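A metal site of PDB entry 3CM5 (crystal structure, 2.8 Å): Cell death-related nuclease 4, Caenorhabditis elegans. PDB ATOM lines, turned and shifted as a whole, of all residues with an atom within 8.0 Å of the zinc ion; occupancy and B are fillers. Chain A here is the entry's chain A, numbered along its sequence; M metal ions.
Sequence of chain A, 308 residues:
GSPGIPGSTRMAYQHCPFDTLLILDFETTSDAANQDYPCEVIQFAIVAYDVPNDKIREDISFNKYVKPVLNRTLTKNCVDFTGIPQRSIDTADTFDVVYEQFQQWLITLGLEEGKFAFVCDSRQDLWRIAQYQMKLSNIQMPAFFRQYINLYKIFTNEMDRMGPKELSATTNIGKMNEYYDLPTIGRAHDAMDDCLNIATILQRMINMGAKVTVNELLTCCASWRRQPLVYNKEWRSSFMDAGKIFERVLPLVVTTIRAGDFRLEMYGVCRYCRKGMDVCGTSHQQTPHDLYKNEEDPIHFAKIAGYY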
ATOM      1  N   ARG A 146       1.343  -4.792  30.000  1.00  0.00           N
ATOM      2  CA  ARG A 146       2.542  -4.201  29.420  1.00  0.00           C
ATOM      3  C   ARG A 146       3.812  -4.480  30.243  1.00  0.00           C
ATOM      4  O   ARG A 146       4.919  -4.022  29.884  1.00  0.00           O
ATOM      5  CB  ARG A 146       2.341  -2.700  29.168  1.00  0.00           C
ATOM      6  CG  ARG A 146       1.425  -2.427  27.991  1.00  0.00           C
ATOM      7  CD  ARG A 146       1.360  -0.969  27.690  1.00  0.00           C
ATOM      8  NE  ARG A 146       2.635  -0.520  27.144  1.00  0.00           N
ATOM      9  CZ  ARG A 146       2.827   0.678  26.604  1.00  0.00           C
ATOM     10  NH1 ARG A 146       1.796   1.525  26.523  1.00  0.00           N
ATOM     11  NH2 ARG A 146       4.024   1.012  26.118  1.00  0.00           N
ATOM     12  N   LEU A 218       6.502  -4.166  27.581  1.00  0.00           N
ATOM     13  CA  LEU A 218       6.056  -3.842  26.257  1.00  0.00           C
ATOM     14  C   LEU A 218       6.272  -2.377  26.024  1.00  0.00           C
ATOM     15  O   LEU A 218       5.709  -1.527  26.709  1.00  0.00           O
ATOM     16  CB  LEU A 218       4.578  -4.211  26.075  1.00  0.00           C
ATOM     17  CG  LEU A 218       4.279  -5.695  25.995  1.00  0.00           C
ATOM     18  CD1 LEU A 218       2.810  -5.897  25.705  1.00  0.00           C
ATOM     19  CD2 LEU A 218       5.135  -6.361  24.942  1.00  0.00           C
ATOM     20  N   THR A 219       7.096  -2.082  25.043  1.00  0.00           N
ATOM     21  CA  THR A 219       7.505  -0.721  24.837  1.00  0.00           C
ATOM     22  C   THR A 219       7.170  -0.253  23.438  1.00  0.00           C
ATOM     23  O   THR A 219       7.126  -1.055  22.504  1.00  0.00           O
ATOM     24  CB  THR A 219       8.986  -0.577  25.184  1.00  0.00           C
ATOM     25  OG1 THR A 219       9.240   0.774  25.536  1.00  0.00           O
ATOM     26  CG2 THR A 219       9.886  -0.996  24.037  1.00  0.00           C
ATOM     27  N   CYS A 220       6.915   1.034  23.302  1.00  0.00           N
ATOM     28  CA  CYS A 220       6.464   1.627  22.045  1.00  0.00           C
ATOM     29  C   CYS A 220       7.575   1.716  20.999  1.00  0.00           C
ATOM     30  O   CYS A 220       7.313   2.153  19.880  1.00  0.00           O
ATOM     31  CB  CYS A 220       5.946   3.038  22.298  1.00  0.00           C
ATOM     32  SG  CYS A 220       7.266   4.189  22.842  1.00  0.00           S
ATOM     33  N   CYS A 221       8.794   1.312  21.339  1.00  0.00           N
ATOM     34  CA  CYS A 221       9.914   1.664  20.477  1.00  0.00           C
ATOM     35  C   CYS A 221      11.210   0.891  20.688  1.00  0.00           C
ATOM     36  O   CYS A 221      11.648   0.673  21.817  1.00  0.00           O
ATOM     37  CB  CYS A 221      10.189   3.141  20.692  1.00  0.00           C
ATOM     38  SG  CYS A 221      10.689   3.925  19.235  1.00  0.00           S
ATOM     39  N   LEU A 252       3.609  -2.332  19.890  1.00  0.00           N
ATOM     40  CA  LEU A 252       4.444  -2.550  21.057  1.00  0.00           C
ATOM     41  C   LEU A 252       5.396  -3.728  20.890  1.00  0.00           C
ATOM     42  O   LEU A 252       4.997  -4.814  20.474  1.00  0.00           O
ATOM     43  CB  LEU A 252       3.590  -2.712  22.317  1.00  0.00           C
ATOM     44  CG  LEU A 252       2.557  -1.604  22.581  1.00  0.00           C
ATOM     45  CD1 LEU A 252       2.100  -1.635  24.003  1.00  0.00           C
ATOM     46  CD2 LEU A 252       3.060  -0.202  22.219  1.00  0.00           C
ATOM     47  N   VAL A 269       4.342   2.944  33.359  1.00  0.00           N
ATOM     48  CA  VAL A 269       4.984   3.954  32.504  1.00  0.00           C
ATOM     49  C   VAL A 269       5.831   3.205  31.488  1.00  0.00           C
ATOM     50  O   VAL A 269       6.394   2.151  31.798  1.00  0.00           O
ATOM     51  CB  VAL A 269       5.835   5.038  33.310  1.00  0.00           C
ATOM     52  CG1 VAL A 269       5.065   5.553  34.520  1.00  0.00           C
ATOM     53  CG2 VAL A 269       7.224   4.510  33.732  1.00  0.00           C
ATOM     54  N   CYS A 270       5.925   3.754  30.283  1.00  0.00           N
ATOM     55  CA  CYS A 270       6.623   3.083  29.213  1.00  0.00           C
ATOM     56  C   CYS A 270       8.142   3.106  29.393  1.00  0.00           C
ATOM     57  O   CYS A 270       8.703   4.182  29.576  1.00  0.00           O
ATOM     58  CB  CYS A 270       6.225   3.709  27.885  1.00  0.00           C
ATOM     59  SG  CYS A 270       7.218   3.130  26.512  1.00  0.00           S
ATOM     60  N   ARG A 271       8.786   1.931  29.348  1.00  0.00           N
ATOM     61  CA  ARG A 271      10.253   1.823  29.560  1.00  0.00           C
ATOM     62  C   ARG A 271      11.128   2.640  28.622  1.00  0.00           C
ATOM     63  O   ARG A 271      12.278   2.931  28.960  1.00  0.00           O
ATOM     64  CB  ARG A 271      10.767   0.384  29.563  1.00  0.00           C
ATOM     65  CG  ARG A 271      11.105  -0.188  30.947  1.00  0.00           C
ATOM     66  CD  ARG A 271      12.214   0.569  31.726  1.00  0.00           C
ATOM     67  NE  ARG A 271      11.766   1.707  32.586  1.00  0.00           N
ATOM     68  CZ  ARG A 271      10.512   1.987  32.982  1.00  0.00           C
ATOM     69  NH1 ARG A 271       9.467   1.226  32.655  1.00  0.00           N
ATOM     70  NH2 ARG A 271      10.289   3.063  33.740  1.00  0.00           N
ATOM     71  N   TYR A 272      10.596   3.002  27.453  1.00  0.00           N
ATOM     72  CA  TYR A 272      11.335   3.808  26.490  1.00  0.00           C
ATOM     73  C   TYR A 272      11.020   5.300  26.607  1.00  0.00           C
ATOM     74  O   TYR A 272      11.893   6.089  26.952  1.00  0.00           O
ATOM     75  CB  TYR A 272      11.118   3.290  25.070  1.00  0.00           C
ATOM     76  CG  TYR A 272      11.961   3.976  24.006  1.00  0.00           C
ATOM     77  CD1 TYR A 272      13.243   3.496  23.682  1.00  0.00           C
ATOM     78  CD2 TYR A 272      11.474   5.114  23.328  1.00  0.00           C
ATOM     79  CE1 TYR A 272      14.031   4.129  22.712  1.00  0.00           C
ATOM     80  CE2 TYR A 272      12.254   5.749  22.356  1.00  0.00           C
ATOM     81  CZ  TYR A 272      13.528   5.257  22.046  1.00  0.00           C
ATOM     82  OH  TYR A 272      14.290   5.881  21.085  1.00  0.00           O
ATOM     83  N   CYS A 273       9.759   5.660  26.334  1.00  0.00           N
ATOM     84  CA  CYS A 273       9.352   7.051  26.206  1.00  0.00           C
ATOM     85  C   CYS A 273       8.826   7.642  27.510  1.00  0.00           C
ATOM     86  O   CYS A 273       8.342   8.792  27.547  1.00  0.00           O
ATOM     87  CB  CYS A 273       8.259   7.177  25.137  1.00  0.00           C
ATOM     88  SG  CYS A 273       6.616   6.796  25.800  1.00  0.00           S
ATOM     89  N   ARG A 274       8.885   6.851  28.578  1.00  0.00           N
ATOM     90  CA  ARG A 274       8.595   7.329  29.939  1.00  0.00           C
ATOM     91  C   ARG A 274       7.276   8.094  30.117  1.00  0.00           C
ATOM     92  O   ARG A 274       7.113   8.811  31.097  1.00  0.00           O
ATOM     93  CB  ARG A 274       9.753   8.190  30.450  1.00  0.00           C
ATOM     94  CG  ARG A 274      11.101   7.581  30.194  1.00  0.00           C
ATOM     95  CD  ARG A 274      11.576   6.752  31.377  1.00  0.00           C
ATOM     96  NE  ARG A 274      12.456   5.664  30.938  1.00  0.00           N
ATOM     97  CZ  ARG A 274      13.407   5.109  31.686  1.00  0.00           C
ATOM     98  NH1 ARG A 274      13.627   5.557  32.922  1.00  0.00           N
ATOM     99  NH2 ARG A 274      14.146   4.125  31.191  1.00  0.00           N
ATOM    100  N   LYS A 275       6.332   7.952  29.195  1.00  0.00           N
ATOM    101  CA  LYS A 275       5.018   8.549  29.374  1.00  0.00           C
ATOM    102  C   LYS A 275       4.051   7.532  29.999  1.00  0.00           C
ATOM    103  O   LYS A 275       4.376   6.336  30.121  1.00  0.00           O
ATOM    104  CB  LYS A 275       4.470   9.088  28.050  1.00  0.00           C
ATOM    105  CG  LYS A 275       5.360  10.121  27.371  1.00  0.00           C
ATOM    106  CD  LYS A 275       4.945  10.394  25.921  1.00  0.00           C
ATOM    107  CE  LYS A 275       5.991  11.270  25.220  1.00  0.00           C
ATOM    108  NZ  LYS A 275       5.780  11.375  23.751  1.00  0.00           N
ATOM    109  N   GLY A 276       2.878   8.005  30.415  1.00  0.00           N
ATOM    110  CA  GLY A 276       1.847   7.147  30.985  1.00  0.00           C
ATOM    111  C   GLY A 276       1.289   6.202  29.943  1.00  0.00           C
ATOM    112  O   GLY A 276       1.327   6.495  28.732  1.00  0.00           O
ATOM    113  N   MET A 277       0.752   5.070  30.400  1.00  0.00           N
ATOM    114  CA  MET A 277       0.317   3.986  29.474  1.00  0.00           C
ATOM    115  C   MET A 277      -1.134   4.124  28.973  1.00  0.00           C
ATOM    116  O   MET A 277      -1.693   3.198  28.368  1.00  0.00           O
ATOM    117  CB  MET A 277       0.615   2.567  30.042  1.00  0.00           C
ATOM    118  CG  MET A 277       2.110   2.213  29.908  1.00  0.00           C
ATOM    119  SD  MET A 277       2.374   0.529  30.657  1.00  0.00           S
ATOM    120  CE  MET A 277       4.224   0.209  30.484  1.00  0.00           C
ATOM    121  N   VAL A 279      -1.415   7.246  27.536  1.00  0.00           N
ATOM    122  CA  VAL A 279      -0.936   8.200  26.520  1.00  0.00           C
ATOM    123  C   VAL A 279       0.097   7.604  25.533  1.00  0.00           C
ATOM    124  O   VAL A 279       0.405   8.205  24.497  1.00  0.00           O
ATOM    125  CB  VAL A 279      -0.355   9.495  27.179  1.00  0.00           C
ATOM    126  CG1 VAL A 279       0.169  10.479  26.113  1.00  0.00           C
ATOM    127  CG2 VAL A 279      -1.402  10.162  28.063  1.00  0.00           C
ATOM    128  N   CYS A 280       0.635   6.426  25.867  1.00  0.00           N
ATOM    129  CA  CYS A 280       1.603   5.758  24.996  1.00  0.00           C
ATOM    130  C   CYS A 280       0.987   4.525  24.385  1.00  0.00           C
ATOM    131  O   CYS A 280       0.247   3.790  25.041  1.00  0.00           O
ATOM    132  CB  CYS A 280       2.868   5.390  25.770  1.00  0.00           C
ATOM    133  SG  CYS A 280       3.897   4.225  24.895  1.00  0.00           S
ATOM    134  N   GLY A 281       1.311   4.284  23.115  1.00  0.00           N
ATOM    135  CA  GLY A 281       0.745   3.164  22.400  1.00  0.00           C
ATOM    136  C   GLY A 281      -0.747   3.318  22.130  1.00  0.00           C
ATOM    137  O   GLY A 281      -1.531   2.402  22.372  1.00  0.00           O
ATOM    138  N   SER A 283      -0.946   4.531  19.177  1.00  0.00           N
ATOM    139  CA  SER A 283      -0.538   4.826  17.824  1.00  0.00           C
ATOM    140  C   SER A 283       0.886   4.269  17.539  1.00  0.00           C
ATOM    141  O   SER A 283       1.804   4.447  18.336  1.00  0.00           O
ATOM    142  CB  SER A 283      -0.579   6.343  17.655  1.00  0.00           C
ATOM    143  OG  SER A 283      -0.048   6.739  16.423  1.00  0.00           O
ATOM    144  N   GLN A 285       4.602   3.816  16.555  1.00  0.00           N
ATOM    145  CA  GLN A 285       5.677   4.796  16.519  1.00  0.00           C
ATOM    146  C   GLN A 285       6.749   4.472  15.471  1.00  0.00           C
ATOM    147  O   GLN A 285       7.594   5.310  15.154  1.00  0.00           O
ATOM    148  CB  GLN A 285       6.308   4.948  17.903  1.00  0.00           C
ATOM    149  CG  GLN A 285       5.413   5.586  18.955  1.00  0.00           C
ATOM    150  CD  GLN A 285       4.871   6.942  18.530  1.00  0.00           C
ATOM    151  OE1 GLN A 285       3.655   7.131  18.391  1.00  0.00           O
ATOM    152  NE2 GLN A 285       5.760   7.908  18.329  1.00  0.00           N
HETATM  153 ZN    ZN M   1       6.183   4.499  24.983  1.00  0.00          ZN
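The side-chain hydroxyl (OG1) of Thr 219 sits close to the side-chain sulfur (SG) of Cys 270 (3.3 Å). SG of Cys 270 lies close to N of Tyr 272, 3.5 Å away. The backbone NH (N) of Cys 270 sits at hydrogen-bond distance from the backbone carbonyl oxygen (O) of Lys 275, at 3.0 Å. NH1 of Arg 146 sits at hydrogen-bond distance from O of Cys 280, 3.1 Å away. The backbone NH (N) of Lys 275 lies close to the side-chain sulfur (SG) of Cys 273, 3.6 Å away.
Of the 20 residues printed, 4 come within 4 Å of the zinc ion.
The zinc ion is bound by SG of Cys 270 (2.3 Å), SG of Cys 280 (2.3 Å), SG of Cys 220 (2.4 Å) and SG of Cys 273 (2.5 Å). The zinc ion has four donor atoms within binding distance.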
